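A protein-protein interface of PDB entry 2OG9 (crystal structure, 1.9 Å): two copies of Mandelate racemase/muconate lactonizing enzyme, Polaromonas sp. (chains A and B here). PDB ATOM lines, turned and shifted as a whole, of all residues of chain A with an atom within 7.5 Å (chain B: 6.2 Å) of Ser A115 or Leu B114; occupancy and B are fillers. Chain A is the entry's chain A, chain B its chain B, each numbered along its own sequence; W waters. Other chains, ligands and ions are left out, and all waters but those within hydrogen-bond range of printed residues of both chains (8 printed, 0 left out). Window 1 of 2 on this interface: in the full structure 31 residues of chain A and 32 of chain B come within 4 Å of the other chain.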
ATOM      1  N   GLY A  75      22.741  -2.712  15.539  1.00  0.00           N
ATOM      2  CA  GLY A  75      21.933  -3.863  15.896  1.00  0.00           C
ATOM      3  C   GLY A  75      21.579  -4.726  14.699  1.00  0.00           C
ATOM      4  O   GLY A  75      21.629  -5.952  14.782  1.00  0.00           O
ATOM      5  N   GLN A  76      21.214  -4.088  13.586  1.00  0.00           N
ATOM      6  CA  GLN A  76      20.861  -4.822  12.377  1.00  0.00           C
ATOM      7  C   GLN A  76      22.046  -5.623  11.866  1.00  0.00           C
ATOM      8  O   GLN A  76      21.909  -6.788  11.502  1.00  0.00           O
ATOM      9  CB  GLN A  76      20.401  -3.871  11.266  1.00  0.00           C
ATOM     10  CG  GLN A  76      19.060  -3.185  11.495  1.00  0.00           C
ATOM     11  CD  GLN A  76      18.599  -2.423  10.257  1.00  0.00           C
ATOM     12  OE1 GLN A  76      19.360  -2.262   9.304  1.00  0.00           O
ATOM     13  NE2 GLN A  76      17.357  -1.954  10.269  1.00  0.00           N
ATOM     14  N   ALA A  78      24.804  -6.644  13.524  1.00  0.00           N
ATOM     15  CA  ALA A  78      25.146  -7.690  14.477  1.00  0.00           C
ATOM     16  C   ALA A  78      24.242  -8.901  14.321  1.00  0.00           C
ATOM     17  O   ALA A  78      24.714 -10.035  14.329  1.00  0.00           O
ATOM     18  CB  ALA A  78      25.061  -7.151  15.902  1.00  0.00           C
ATOM     19  N   HIS A  79      22.940  -8.667  14.176  1.00  0.00           N
ATOM     20  CA  HIS A  79      22.011  -9.781  14.020  1.00  0.00           C
ATOM     21  C   HIS A  79      22.207 -10.462  12.665  1.00  0.00           C
ATOM     22  O   HIS A  79      22.229 -11.693  12.574  1.00  0.00           O
ATOM     23  CB  HIS A  79      20.561  -9.305  14.156  1.00  0.00           C
ATOM     24  CG  HIS A  79      19.592 -10.423  14.392  1.00  0.00           C
ATOM     25  ND1 HIS A  79      19.554 -11.135  15.571  1.00  0.00           N
ATOM     26  CD2 HIS A  79      18.658 -10.979  13.585  1.00  0.00           C
ATOM     27  CE1 HIS A  79      18.638 -12.083  15.482  1.00  0.00           C
ATOM     28  NE2 HIS A  79      18.079 -12.010  14.286  1.00  0.00           N
ATOM     29  N   ALA A  80      22.355  -9.661  11.613  1.00  0.00           N
ATOM     30  CA  ALA A  80      22.562 -10.198  10.273  1.00  0.00           C
ATOM     31  C   ALA A  80      23.782 -11.121  10.270  1.00  0.00           C
ATOM     32  O   ALA A  80      23.757 -12.199   9.678  1.00  0.00           O
ATOM     33  CB  ALA A  80      22.767  -9.057   9.273  1.00  0.00           C
ATOM     34  N   GLU A  82      25.069 -12.747  12.815  1.00  0.00           N
ATOM     35  CA  GLU A  82      24.806 -13.953  13.587  1.00  0.00           C
ATOM     36  C   GLU A  82      23.941 -14.984  12.871  1.00  0.00           C
ATOM     37  O   GLU A  82      24.151 -16.182  13.038  1.00  0.00           O
ATOM     38  CB  GLU A  82      24.171 -13.586  14.930  1.00  0.00           C
ATOM     39  CG  GLU A  82      23.878 -14.783  15.816  1.00  0.00           C
ATOM     40  CD  GLU A  82      23.365 -14.378  17.184  1.00  0.00           C
ATOM     41  OE1 GLU A  82      22.634 -13.371  17.269  1.00  0.00           O
ATOM     42  OE2 GLU A  82      23.681 -15.072  18.175  1.00  0.00           O
ATOM     43  N   ILE A  83      22.983 -14.540  12.061  1.00  0.00           N
ATOM     44  CA  ILE A  83      22.115 -15.494  11.373  1.00  0.00           C
ATOM     45  C   ILE A  83      22.536 -15.844   9.947  1.00  0.00           C
ATOM     46  O   ILE A  83      22.057 -16.828   9.387  1.00  0.00           O
ATOM     47  CB  ILE A  83      20.636 -15.008  11.363  1.00  0.00           C
ATOM     48  CG1 ILE A  83      20.476 -13.768  10.481  1.00  0.00           C
ATOM     49  CG2 ILE A  83      20.194 -14.681  12.790  1.00  0.00           C
ATOM     50  CD1 ILE A  83      19.033 -13.256  10.416  1.00  0.00           C
ATOM     51  N   TRP A  99      12.903 -16.923   4.773  1.00  0.00           N
ATOM     52  CA  TRP A  99      12.555 -15.775   5.613  1.00  0.00           C
ATOM     53  C   TRP A  99      12.141 -16.373   6.972  1.00  0.00           C
ATOM     54  O   TRP A  99      12.588 -15.923   8.033  1.00  0.00           O
ATOM     55  CB  TRP A  99      11.374 -14.999   5.014  1.00  0.00           C
ATOM     56  CG  TRP A  99      11.169 -13.628   5.627  1.00  0.00           C
ATOM     57  CD1 TRP A  99      11.674 -12.443   5.173  1.00  0.00           C
ATOM     58  CD2 TRP A  99      10.430 -13.316   6.820  1.00  0.00           C
ATOM     59  NE1 TRP A  99      11.296 -11.415   6.007  1.00  0.00           N
ATOM     60  CE2 TRP A  99      10.535 -11.923   7.026  1.00  0.00           C
ATOM     61  CE3 TRP A  99       9.694 -14.082   7.735  1.00  0.00           C
ATOM     62  CZ2 TRP A  99       9.928 -11.275   8.108  1.00  0.00           C
ATOM     63  CZ3 TRP A  99       9.090 -13.439   8.811  1.00  0.00           C
ATOM     64  CH2 TRP A  99       9.214 -12.048   8.988  1.00  0.00           C
ATOM     65  N   LEU A 102      15.143 -17.952   8.987  1.00  0.00           N
ATOM     66  CA  LEU A 102      15.966 -16.952   9.660  1.00  0.00           C
ATOM     67  C   LEU A 102      15.228 -16.332  10.839  1.00  0.00           C
ATOM     68  O   LEU A 102      15.841 -15.978  11.853  1.00  0.00           O
ATOM     69  CB  LEU A 102      16.393 -15.857   8.680  1.00  0.00           C
ATOM     70  CG  LEU A 102      17.401 -16.280   7.604  1.00  0.00           C
ATOM     71  CD1 LEU A 102      17.842 -15.055   6.820  1.00  0.00           C
ATOM     72  CD2 LEU A 102      18.603 -16.954   8.243  1.00  0.00           C
ATOM     73  N   CYS A 103      13.912 -16.203  10.711  1.00  0.00           N
ATOM     74  CA  CYS A 103      13.108 -15.637  11.788  1.00  0.00           C
ATOM     75  C   CYS A 103      13.109 -16.640  12.948  1.00  0.00           C
ATOM     76  O   CYS A 103      13.257 -16.259  14.112  1.00  0.00           O
ATOM     77  CB  CYS A 103      11.679 -15.381  11.297  1.00  0.00           C
ATOM     78  SG  CYS A 103      10.658 -14.385  12.416  1.00  0.00           S
ATOM     79  N   GLY A 106      16.039 -16.755  15.191  1.00  0.00           N
ATOM     80  CA  GLY A 106      16.092 -15.708  16.199  1.00  0.00           C
ATOM     81  C   GLY A 106      14.691 -15.471  16.730  1.00  0.00           C
ATOM     82  O   GLY A 106      14.269 -14.328  16.922  1.00  0.00           O
ATOM     83  N   ALA A 107      13.976 -16.564  16.980  1.00  0.00           N
ATOM     84  CA  ALA A 107      12.597 -16.507  17.451  1.00  0.00           C
ATOM     85  C   ALA A 107      12.340 -15.657  18.691  1.00  0.00           C
ATOM     86  O   ALA A 107      11.287 -15.031  18.796  1.00  0.00           O
ATOM     87  CB  ALA A 107      12.066 -17.924  17.681  1.00  0.00           C
ATOM     88  N   SER A 108      13.271 -15.623  19.638  1.00  0.00           N
ATOM     89  CA  SER A 108      13.016 -14.826  20.830  1.00  0.00           C
ATOM     90  C   SER A 108      13.068 -13.332  20.512  1.00  0.00           C
ATOM     91  O   SER A 108      12.735 -12.506  21.355  1.00  0.00           O
ATOM     92  CB  SER A 108      14.003 -15.176  21.957  1.00  0.00           C
ATOM     93  OG  SER A 108      15.256 -14.547  21.801  1.00  0.00           O
ATOM     94  N   ALA A 109      13.469 -12.997  19.289  1.00  0.00           N
ATOM     95  CA  ALA A 109      13.556 -11.604  18.853  1.00  0.00           C
ATOM     96  C   ALA A 109      12.250 -11.118  18.221  1.00  0.00           C
ATOM     97  O   ALA A 109      12.098  -9.930  17.939  1.00  0.00           O
ATOM     98  CB  ALA A 109      14.714 -11.432  17.867  1.00  0.00           C
ATOM     99  N   GLY A 110      11.314 -12.032  17.985  1.00  0.00           N
ATOM    100  CA  GLY A 110      10.036 -11.643  17.412  1.00  0.00           C
ATOM    101  C   GLY A 110       9.952 -11.596  15.893  1.00  0.00           C
ATOM    102  O   GLY A 110      10.879 -11.999  15.190  1.00  0.00           O
ATOM    103  N   ARG A 111       8.831 -11.092  15.390  1.00  0.00           N
ATOM    104  CA  ARG A 111       8.599 -11.004  13.953  1.00  0.00           C
ATOM    105  C   ARG A 111       8.626  -9.581  13.411  1.00  0.00           C
ATOM    106  O   ARG A 111       8.085  -9.317  12.335  1.00  0.00           O
ATOM    107  CB  ARG A 111       7.252 -11.630  13.596  1.00  0.00           C
ATOM    108  CG  ARG A 111       7.152 -13.115  13.834  1.00  0.00           C
ATOM    109  CD  ARG A 111       5.812 -13.610  13.312  1.00  0.00           C
ATOM    110  NE  ARG A 111       5.637 -15.053  13.449  1.00  0.00           N
ATOM    111  CZ  ARG A 111       4.559 -15.706  13.024  1.00  0.00           C
ATOM    112  NH1 ARG A 111       3.570 -15.039  12.440  1.00  0.00           N
ATOM    113  NH2 ARG A 111       4.466 -17.020  13.188  1.00  0.00           N
ATOM    114  N   SER A 112       9.244  -8.667  14.146  1.00  0.00           N
ATOM    115  CA  SER A 112       9.319  -7.283  13.700  1.00  0.00           C
ATOM    116  C   SER A 112      10.500  -6.592  14.346  1.00  0.00           C
ATOM    117  O   SER A 112      11.076  -7.099  15.306  1.00  0.00           O
ATOM    118  CB  SER A 112       8.040  -6.531  14.067  1.00  0.00           C
ATOM    119  OG  SER A 112       7.938  -6.377  15.468  1.00  0.00           O
ATOM    120  N   GLY A 113      10.861  -5.428  13.820  1.00  0.00           N
ATOM    121  CA  GLY A 113      11.974  -4.699  14.395  1.00  0.00           C
ATOM    122  C   GLY A 113      13.316  -5.008  13.766  1.00  0.00           C
ATOM    123  O   GLY A 113      13.390  -5.444  12.616  1.00  0.00           O
ATOM    124  N   LEU A 114      14.380  -4.797  14.531  1.00  0.00           N
ATOM    125  CA  LEU A 114      15.738  -5.008  14.039  1.00  0.00           C
ATOM    126  C   LEU A 114      16.050  -6.381  13.449  1.00  0.00           C
ATOM    127  O   LEU A 114      16.738  -6.467  12.432  1.00  0.00           O
ATOM    128  CB  LEU A 114      16.759  -4.706  15.143  1.00  0.00           C
ATOM    129  CG  LEU A 114      16.807  -3.285  15.712  1.00  0.00           C
ATOM    130  CD1 LEU A 114      17.896  -3.200  16.777  1.00  0.00           C
ATOM    131  CD2 LEU A 114      17.082  -2.281  14.597  1.00  0.00           C
ATOM    132  N   SER A 115      15.563  -7.453  14.069  1.00  0.00           N
ATOM    133  CA  SER A 115      15.872  -8.784  13.556  1.00  0.00           C
ATOM    134  C   SER A 115      15.264  -9.054  12.180  1.00  0.00           C
ATOM    135  O   SER A 115      15.940  -9.578  11.295  1.00  0.00           O
ATOM    136  CB  SER A 115      15.425  -9.861  14.547  1.00  0.00           C
ATOM    137  OG  SER A 115      14.029  -9.807  14.763  1.00  0.00           O
ATOM    138  N   THR A 116      14.000  -8.689  11.984  1.00  0.00           N
ATOM    139  CA  THR A 116      13.378  -8.929  10.693  1.00  0.00           C
ATOM    140  C   THR A 116      13.876  -7.945   9.633  1.00  0.00           C
ATOM    141  O   THR A 116      13.827  -8.238   8.443  1.00  0.00           O
ATOM    142  CB  THR A 116      11.829  -8.894  10.791  1.00  0.00           C
ATOM    143  OG1 THR A 116      11.419  -7.756  11.545  1.00  0.00           O
ATOM    144  CG2 THR A 116      11.312 -10.160  11.464  1.00  0.00           C
ATOM    145  N   GLN A 117      14.357  -6.781  10.059  1.00  0.00           N
ATOM    146  CA  GLN A 117      14.893  -5.811   9.102  1.00  0.00           C
ATOM    147  C   GLN A 117      16.217  -6.378   8.591  1.00  0.00           C
ATOM    148  O   GLN A 117      16.565  -6.226   7.422  1.00  0.00           O
ATOM    149  CB  GLN A 117      15.088  -4.447   9.774  1.00  0.00           C
ATOM    150  CG  GLN A 117      13.766  -3.880  10.287  1.00  0.00           C
ATOM    151  CD  GLN A 117      13.892  -2.536  10.982  1.00  0.00           C
ATOM    152  OE1 GLN A 117      14.963  -2.166  11.479  1.00  0.00           O
ATOM    153  NE2 GLN A 117      12.775  -1.807  11.051  1.00  0.00           N
ATOM    154  N   ALA A 118      16.950  -7.052   9.469  1.00  0.00           N
ATOM    155  CA  ALA A 118      18.207  -7.675   9.069  1.00  0.00           C
ATOM    156  C   ALA A 118      17.849  -8.767   8.054  1.00  0.00           C
ATOM    157  O   ALA A 118      18.477  -8.897   6.997  1.00  0.00           O
ATOM    158  CB  ALA A 118      18.900  -8.278  10.290  1.00  0.00           C
ATOM    159  N   ILE A 119      16.824  -9.545   8.378  1.00  0.00           N
ATOM    160  CA  ILE A 119      16.364 -10.609   7.493  1.00  0.00           C
ATOM    161  C   ILE A 119      15.978 -10.015   6.131  1.00  0.00           C
ATOM    162  O   ILE A 119      16.251 -10.602   5.083  1.00  0.00           O
ATOM    163  CB  ILE A 119      15.146 -11.350   8.117  1.00  0.00           C
ATOM    164  CG1 ILE A 119      15.607 -12.167   9.330  1.00  0.00           C
ATOM    165  CG2 ILE A 119      14.482 -12.252   7.087  1.00  0.00           C
ATOM    166  CD1 ILE A 119      14.463 -12.864  10.087  1.00  0.00           C
ATOM    167  N   GLY A 120      15.355  -8.842   6.163  1.00  0.00           N
ATOM    168  CA  GLY A 120      14.932  -8.174   4.943  1.00  0.00           C
ATOM    169  C   GLY A 120      16.052  -7.880   3.957  1.00  0.00           C
ATOM    170  O   GLY A 120      15.823  -7.893   2.752  1.00  0.00           O
ATOM    171  N   ALA A 121      17.254  -7.605   4.452  1.00  0.00           N
ATOM    172  CA  ALA A 121      18.373  -7.328   3.553  1.00  0.00           C
ATOM    173  C   ALA A 121      18.645  -8.573   2.717  1.00  0.00           C
ATOM    174  O   ALA A 121      18.902  -8.478   1.508  1.00  0.00           O
ATOM    175  CB  ALA A 121      19.617  -6.945   4.348  1.00  0.00           C
ATOM    176  N   PHE A 122      18.581  -9.738   3.365  1.00  0.00           N
ATOM    177  CA  PHE A 122      18.809 -11.011   2.689  1.00  0.00           C
ATOM    178  C   PHE A 122      17.638 -11.298   1.754  1.00  0.00           C
ATOM    179  O   PHE A 122      17.825 -11.740   0.624  1.00  0.00           O
ATOM    180  CB  PHE A 122      18.925 -12.161   3.707  1.00  0.00           C
ATOM    181  CG  PHE A 122      20.094 -12.035   4.653  1.00  0.00           C
ATOM    182  CD1 PHE A 122      21.397 -12.006   4.172  1.00  0.00           C
ATOM    183  CD2 PHE A 122      19.885 -11.938   6.027  1.00  0.00           C
ATOM    184  CE1 PHE A 122      22.483 -11.880   5.050  1.00  0.00           C
ATOM    185  CE2 PHE A 122      20.963 -11.811   6.915  1.00  0.00           C
ATOM    186  CZ  PHE A 122      22.264 -11.782   6.421  1.00  0.00           C
ATOM    187  N   GLY A 293      10.691  -5.798   6.842  1.00  0.00           N
ATOM    188  CA  GLY A 293      11.315  -7.104   6.718  1.00  0.00           C
ATOM    189  C   GLY A 293      11.591  -7.586   5.308  1.00  0.00           C
ATOM    190  O   GLY A 293      11.846  -8.772   5.099  1.00  0.00           O
ATOM    191  N   SER B  68      18.342 -13.417  25.072  1.00  0.00           N
ATOM    192  CA  SER B  68      18.013 -13.973  23.772  1.00  0.00           C
ATOM    193  C   SER B  68      18.314 -15.461  23.800  1.00  0.00           C
ATOM    194  O   SER B  68      19.417 -15.868  24.176  1.00  0.00           O
ATOM    195  CB  SER B  68      18.848 -13.330  22.657  1.00  0.00           C
ATOM    196  OG  SER B  68      18.640 -11.935  22.592  1.00  0.00           O
ATOM    197  N   ALA B  71      19.606 -16.825  18.278  1.00  0.00           N
ATOM    198  CA  ALA B  71      20.029 -15.525  17.753  1.00  0.00           C
ATOM    199  C   ALA B  71      19.365 -14.298  18.376  1.00  0.00           C
ATOM    200  O   ALA B  71      18.154 -14.261  18.578  1.00  0.00           O
ATOM    201  CB  ALA B  71      19.853 -15.497  16.237  1.00  0.00           C
ATOM    202  N   GLY B  72      20.175 -13.287  18.680  1.00  0.00           N
ATOM    203  CA  GLY B  72      19.641 -12.070  19.263  1.00  0.00           C
ATOM    204  C   GLY B  72      20.583 -11.343  20.201  1.00  0.00           C
ATOM    205  O   GLY B  72      20.509 -10.123  20.320  1.00  0.00           O
ATOM    206  N   GLY B  73      21.461 -12.087  20.871  1.00  0.00           N
ATOM    207  CA  GLY B  73      22.395 -11.487  21.811  1.00  0.00           C
ATOM    208  C   GLY B  73      23.210 -10.338  21.249  1.00  0.00           C
ATOM    209  O   GLY B  73      23.185  -9.233  21.802  1.00  0.00           O
ATOM    210  N   GLY B  75      22.776  -8.485  18.606  1.00  0.00           N
ATOM    211  CA  GLY B  75      21.934  -7.374  18.199  1.00  0.00           C
ATOM    212  C   GLY B  75      21.464  -6.538  19.370  1.00  0.00           C
ATOM    213  O   GLY B  75      21.479  -5.308  19.307  1.00  0.00           O
ATOM    214  N   GLN B  76      21.033  -7.200  20.442  1.00  0.00           N
ATOM    215  CA  GLN B  76      20.573  -6.483  21.624  1.00  0.00           C
ATOM    216  C   GLN B  76      21.696  -5.642  22.211  1.00  0.00           C
ATOM    217  O   GLN B  76      21.490  -4.485  22.571  1.00  0.00           O
ATOM    218  CB  GLN B  76      20.070  -7.460  22.695  1.00  0.00           C
ATOM    219  CG  GLN B  76      18.691  -8.051  22.438  1.00  0.00           C
ATOM    220  CD  GLN B  76      18.254  -8.962  23.576  1.00  0.00           C
ATOM    221  OE1 GLN B  76      18.944  -9.073  24.587  1.00  0.00           O
ATOM    222  NE2 GLN B  76      17.105  -9.609  23.419  1.00  0.00           N
ATOM    223  N   HIS B  79      22.627  -2.544  19.954  1.00  0.00           N
ATOM    224  CA  HIS B  79      21.639  -1.479  20.046  1.00  0.00           C
ATOM    225  C   HIS B  79      21.719  -0.783  21.402  1.00  0.00           C
ATOM    226  O   HIS B  79      21.670   0.448  21.484  1.00  0.00           O
ATOM    227  CB  HIS B  79      20.232  -2.031  19.833  1.00  0.00           C
ATOM    228  CG  HIS B  79      19.226  -0.969  19.523  1.00  0.00           C
ATOM    229  ND1 HIS B  79      19.216  -0.288  18.327  1.00  0.00           N
ATOM    230  CD2 HIS B  79      18.236  -0.431  20.272  1.00  0.00           C
ATOM    231  CE1 HIS B  79      18.261   0.626  18.349  1.00  0.00           C
ATOM    232  NE2 HIS B  79      17.651   0.560  19.519  1.00  0.00           N
ATOM    233  N   SER B 112       8.963  -3.153  19.111  1.00  0.00           N
ATOM    234  CA  SER B 112       9.080  -4.525  19.582  1.00  0.00           C
ATOM    235  C   SER B 112      10.331  -5.156  19.004  1.00  0.00           C
ATOM    236  O   SER B 112      10.946  -4.605  18.091  1.00  0.00           O
ATOM    237  CB  SER B 112       7.858  -5.344  19.166  1.00  0.00           C
ATOM    238  OG  SER B 112       7.850  -5.566  17.770  1.00  0.00           O
ATOM    239  N   GLY B 113      10.710  -6.312  19.534  1.00  0.00           N
ATOM    240  CA  GLY B 113      11.892  -6.979  19.024  1.00  0.00           C
ATOM    241  C   GLY B 113      13.174  -6.614  19.746  1.00  0.00           C
ATOM    242  O   GLY B 113      13.149  -6.185  20.899  1.00  0.00           O
ATOM    243  N   LEU B 114      14.298  -6.774  19.057  1.00  0.00           N
ATOM    244  CA  LEU B 114      15.609  -6.502  19.636  1.00  0.00           C
ATOM    245  C   LEU B 114      15.812  -5.124  20.262  1.00  0.00           C
ATOM    246  O   LEU B 114      16.393  -5.021  21.343  1.00  0.00           O
ATOM    247  CB  LEU B 114      16.706  -6.734  18.591  1.00  0.00           C
ATOM    248  CG  LEU B 114      16.848  -8.156  18.035  1.00  0.00           C
ATOM    249  CD1 LEU B 114      18.014  -8.208  17.057  1.00  0.00           C
ATOM    250  CD2 LEU B 114      17.072  -9.139  19.176  1.00  0.00           C
ATOM    251  N   SER B 115      15.342  -4.066  19.603  1.00  0.00           N
ATOM    252  CA  SER B 115      15.546  -2.722  20.138  1.00  0.00           C
ATOM    253  C   SER B 115      14.830  -2.464  21.462  1.00  0.00           C
ATOM    254  O   SER B 115      15.416  -1.887  22.381  1.00  0.00           O
ATOM    255  CB  SER B 115      15.134  -1.665  19.110  1.00  0.00           C
ATOM    256  OG  SER B 115      13.750  -1.720  18.837  1.00  0.00           O
ATOM    257  N   THR B 116      13.574  -2.883  21.573  1.00  0.00           N
ATOM    258  CA  THR B 116      12.850  -2.662  22.818  1.00  0.00           C
ATOM    259  C   THR B 116      13.307  -3.636  23.907  1.00  0.00           C
ATOM    260  O   THR B 116      13.140  -3.367  25.094  1.00  0.00           O
ATOM    261  CB  THR B 116      11.316  -2.762  22.616  1.00  0.00           C
ATOM    262  OG1 THR B 116      11.004  -3.945  21.881  1.00  0.00           O
ATOM    263  CG2 THR B 116      10.803  -1.541  21.853  1.00  0.00           C
ATOM    264  N   GLN B 117      13.888  -4.763  23.506  1.00  0.00           N
ATOM    265  CA  GLN B 117      14.394  -5.723  24.481  1.00  0.00           C
ATOM    266  C   GLN B 117      15.659  -5.116  25.093  1.00  0.00           C
ATOM    267  O   GLN B 117      15.933  -5.288  26.277  1.00  0.00           O
ATOM    268  CB  GLN B 117      14.680  -7.075  23.812  1.00  0.00           C
ATOM    269  CG  GLN B 117      13.392  -7.765  23.338  1.00  0.00           C
ATOM    270  CD  GLN B 117      13.623  -9.047  22.555  1.00  0.00           C
ATOM    271  OE1 GLN B 117      14.746  -9.352  22.140  1.00  0.00           O
ATOM    272  NE2 GLN B 117      12.544  -9.800  22.329  1.00  0.00           N
ATOM    273  N   ALA B 118      16.421  -4.387  24.284  1.00  0.00           N
ATOM    274  CA  ALA B 118      17.624  -3.727  24.781  1.00  0.00           C
ATOM    275  C   ALA B 118      17.172  -2.636  25.754  1.00  0.00           C
ATOM    276  O   ALA B 118      17.750  -2.457  26.831  1.00  0.00           O
ATOM    277  CB  ALA B 118      18.406  -3.121  23.622  1.00  0.00           C
ATOM    278  N   ILE B 119      16.129  -1.909  25.366  1.00  0.00           N
ATOM    279  CA  ILE B 119      15.568  -0.855  26.204  1.00  0.00           C
ATOM    280  C   ILE B 119      15.103  -1.483  27.523  1.00  0.00           C
ATOM    281  O   ILE B 119      15.266  -0.902  28.593  1.00  0.00           O
ATOM    282  CB  ILE B 119      14.364  -0.175  25.490  1.00  0.00           C
ATOM    283  CG1 ILE B 119      14.872   0.658  24.308  1.00  0.00           C
ATOM    284  CG2 ILE B 119      13.576   0.682  26.471  1.00  0.00           C
ATOM    285  CD1 ILE B 119      13.764   1.311  23.464  1.00  0.00           C
HETATM  286  O   HOH W   1       9.592  -8.268  17.275  1.00  0.00           O
HETATM  287  O   HOH W   2      13.426  -4.005  17.199  1.00  0.00           O
HETATM  288  O   HOH W   3      21.831 -10.849  17.222  1.00  0.00           O
HETATM  289  O   HOH W   4       9.644  -3.501  16.026  1.00  0.00           O
HETATM  290  O   HOH W   5      13.609  -7.557  16.313  1.00  0.00           O
HETATM  291  O   HOH W   6      22.403 -14.771  20.615  1.00  0.00           O
HETATM  292  O   HOH W   7      15.962 -11.950  21.628  1.00  0.00           O
HETATM  293  O   HOH W   8      21.655  -0.454  16.814  1.00  0.00           O
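The backbone carbonyl oxygen (O) of Ser A108 is in hydrogen-bond range of the side-chain amide nitrogen (NE2) of Gln B117, at 2.9 Å. The side-chain hydroxyl (OG) of Ser A112 sits at hydrogen-bond distance from the side-chain hydroxyl (OG) of Ser B112, at 2.4 Å. N of Gly B72 sits at hydrogen-bond distance from OE1 of Glu A82 (2.8 Å).
The side-chain hydroxyl of Ser B68 sits at hydrogen-bond distance from the side-chain amide nitrogen of Gln B76, 2.9 Å away. The side-chain amide oxygen of Gln B117 lies within hydrogen-bond range of the side-chain amide nitrogen of Gln B76. The side-chain hydroxyl of Ser B68 sits at hydrogen-bond distance from the backbone NH of Gly B73 (3.3 Å). The backbone carbonyl oxygen (O) of Gly A113 lies within hydrogen-bond range of the side-chain hydroxyl (OG1) of Thr A116 (3.2 Å). The backbone carbonyl oxygen of Gly B113 sits at hydrogen-bond distance from the side-chain hydroxyl of Thr B116, 3.3 Å away. O of Gly B72 sits close to OG of Ser B68, 3.5 Å away.
CA of Gly B75 touches O of Gly A75, at 3.7 Å. N of Gly B75 touches CB of Ala A78 (3.8 Å). CB of Ala B71 touches CE1 of His A79, at 3.7 Å. Gly B72 touches His A79 (N to CE1, 3.7 Å). OE1 of Glu A82 touches N of Gly B73 (3.9999 Å). Ser A108 touches Ser B68 (OG to CA, 3.4 Å). Ser A112 touches Gly B113 (O to CA, 3.8 Å). CA of Gly A113 touches O of Ser B112, at 3.8 Å. His B79 touches Leu A114 (ND1 to CD1, 3.6 Å). Ser B115 touches Leu A114 (N to CD1, 3.9 Å).
Printed residues of chain B within 4 Å of Ala A78: Gly B75 (3.8 Å). Of the printed residues of chain B, Ser A108 touches Ser B68 (3.4 Å) and Gln B117 (2.9 Å). Arg A111 touches none of the printed residues of chain B. Printed residues of chain B within 4 Å of Ser A115: Leu B114 (3.9 Å). Phe A122 touches none of the printed residues of chain B. Of the printed residues of chain A, Gly B72 touches His A79 and Glu A82. Of the printed residues of chain A, Leu B114 touches His A79 (3.6 Å), Ala A109 (3.5 Å) and Ser A115 (3.9 Å). The nearest residue of chain B that does not touch Ser A115 is Gly B113 (5.5 Å).
Of the 15 printed residues of chain B, 11 touch a printed residue of chain A. Hydrophobic or aromatic side chains of chain A within 4 Å of the printed part of chain B: Ala A78, His A79, Ile A83, Ala A109 and Leu A114.
Gly B75 touches its own counterpart, Gly A75. Ser B112 touches its own counterpart, Ser A112. Ser A112 touches Gly B113, and with the chains exchanged Gly A113 touches Ser B112. Leu A114 touches Ser B115, and with the chains exchanged Ser A115 touches Leu B114. Positions printed for both chains: 75, 76, 79, 112, 113, 114, 115, 116, 117, 118 and 119.
Water W3 lies within hydrogen-bond range of the side-chain carboxylate of Glu A82 (2.6 Å), a ring nitrogen (ND1) of His A79 (2.8 Å), the backbone NH of Gly B75 (2.9 Å) and the backbone NH of Gly B72 (3.3 Å). Water W4 lies within hydrogen-bond range of O of Ser B112 (2.7 Å), N of Gly A113 (3.2 Å) and OG of Ser A112 (3.4 Å). Water W7 lies within hydrogen-bond range of OG of Ser A108 (2.7 Å), OG of Ser B68 (2.8 Å), OE1 of Gln B117 (2.9 Å) and NE2 of Gln B76 (3.2 Å). Water W1 lies within hydrogen-bond range of O of Ser A112 (2.7 Å), O of Ala A109 (3.1 Å), N of Gly B113 (3.2 Å), OG of Ser B112 (3.3 Å) and N of Arg A111 (3.5 Å). Water W6 lies within hydrogen-bond range of the side-chain carboxylate of Glu A82 (2.8 Å), the backbone NH of Gly B73 (2.9 Å) and the backbone NH of Gly B72 (3.3 Å). Water W8 bridges N of Gly A75 (2.8 Å) and ND1 of His B79 (2.9 Å).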
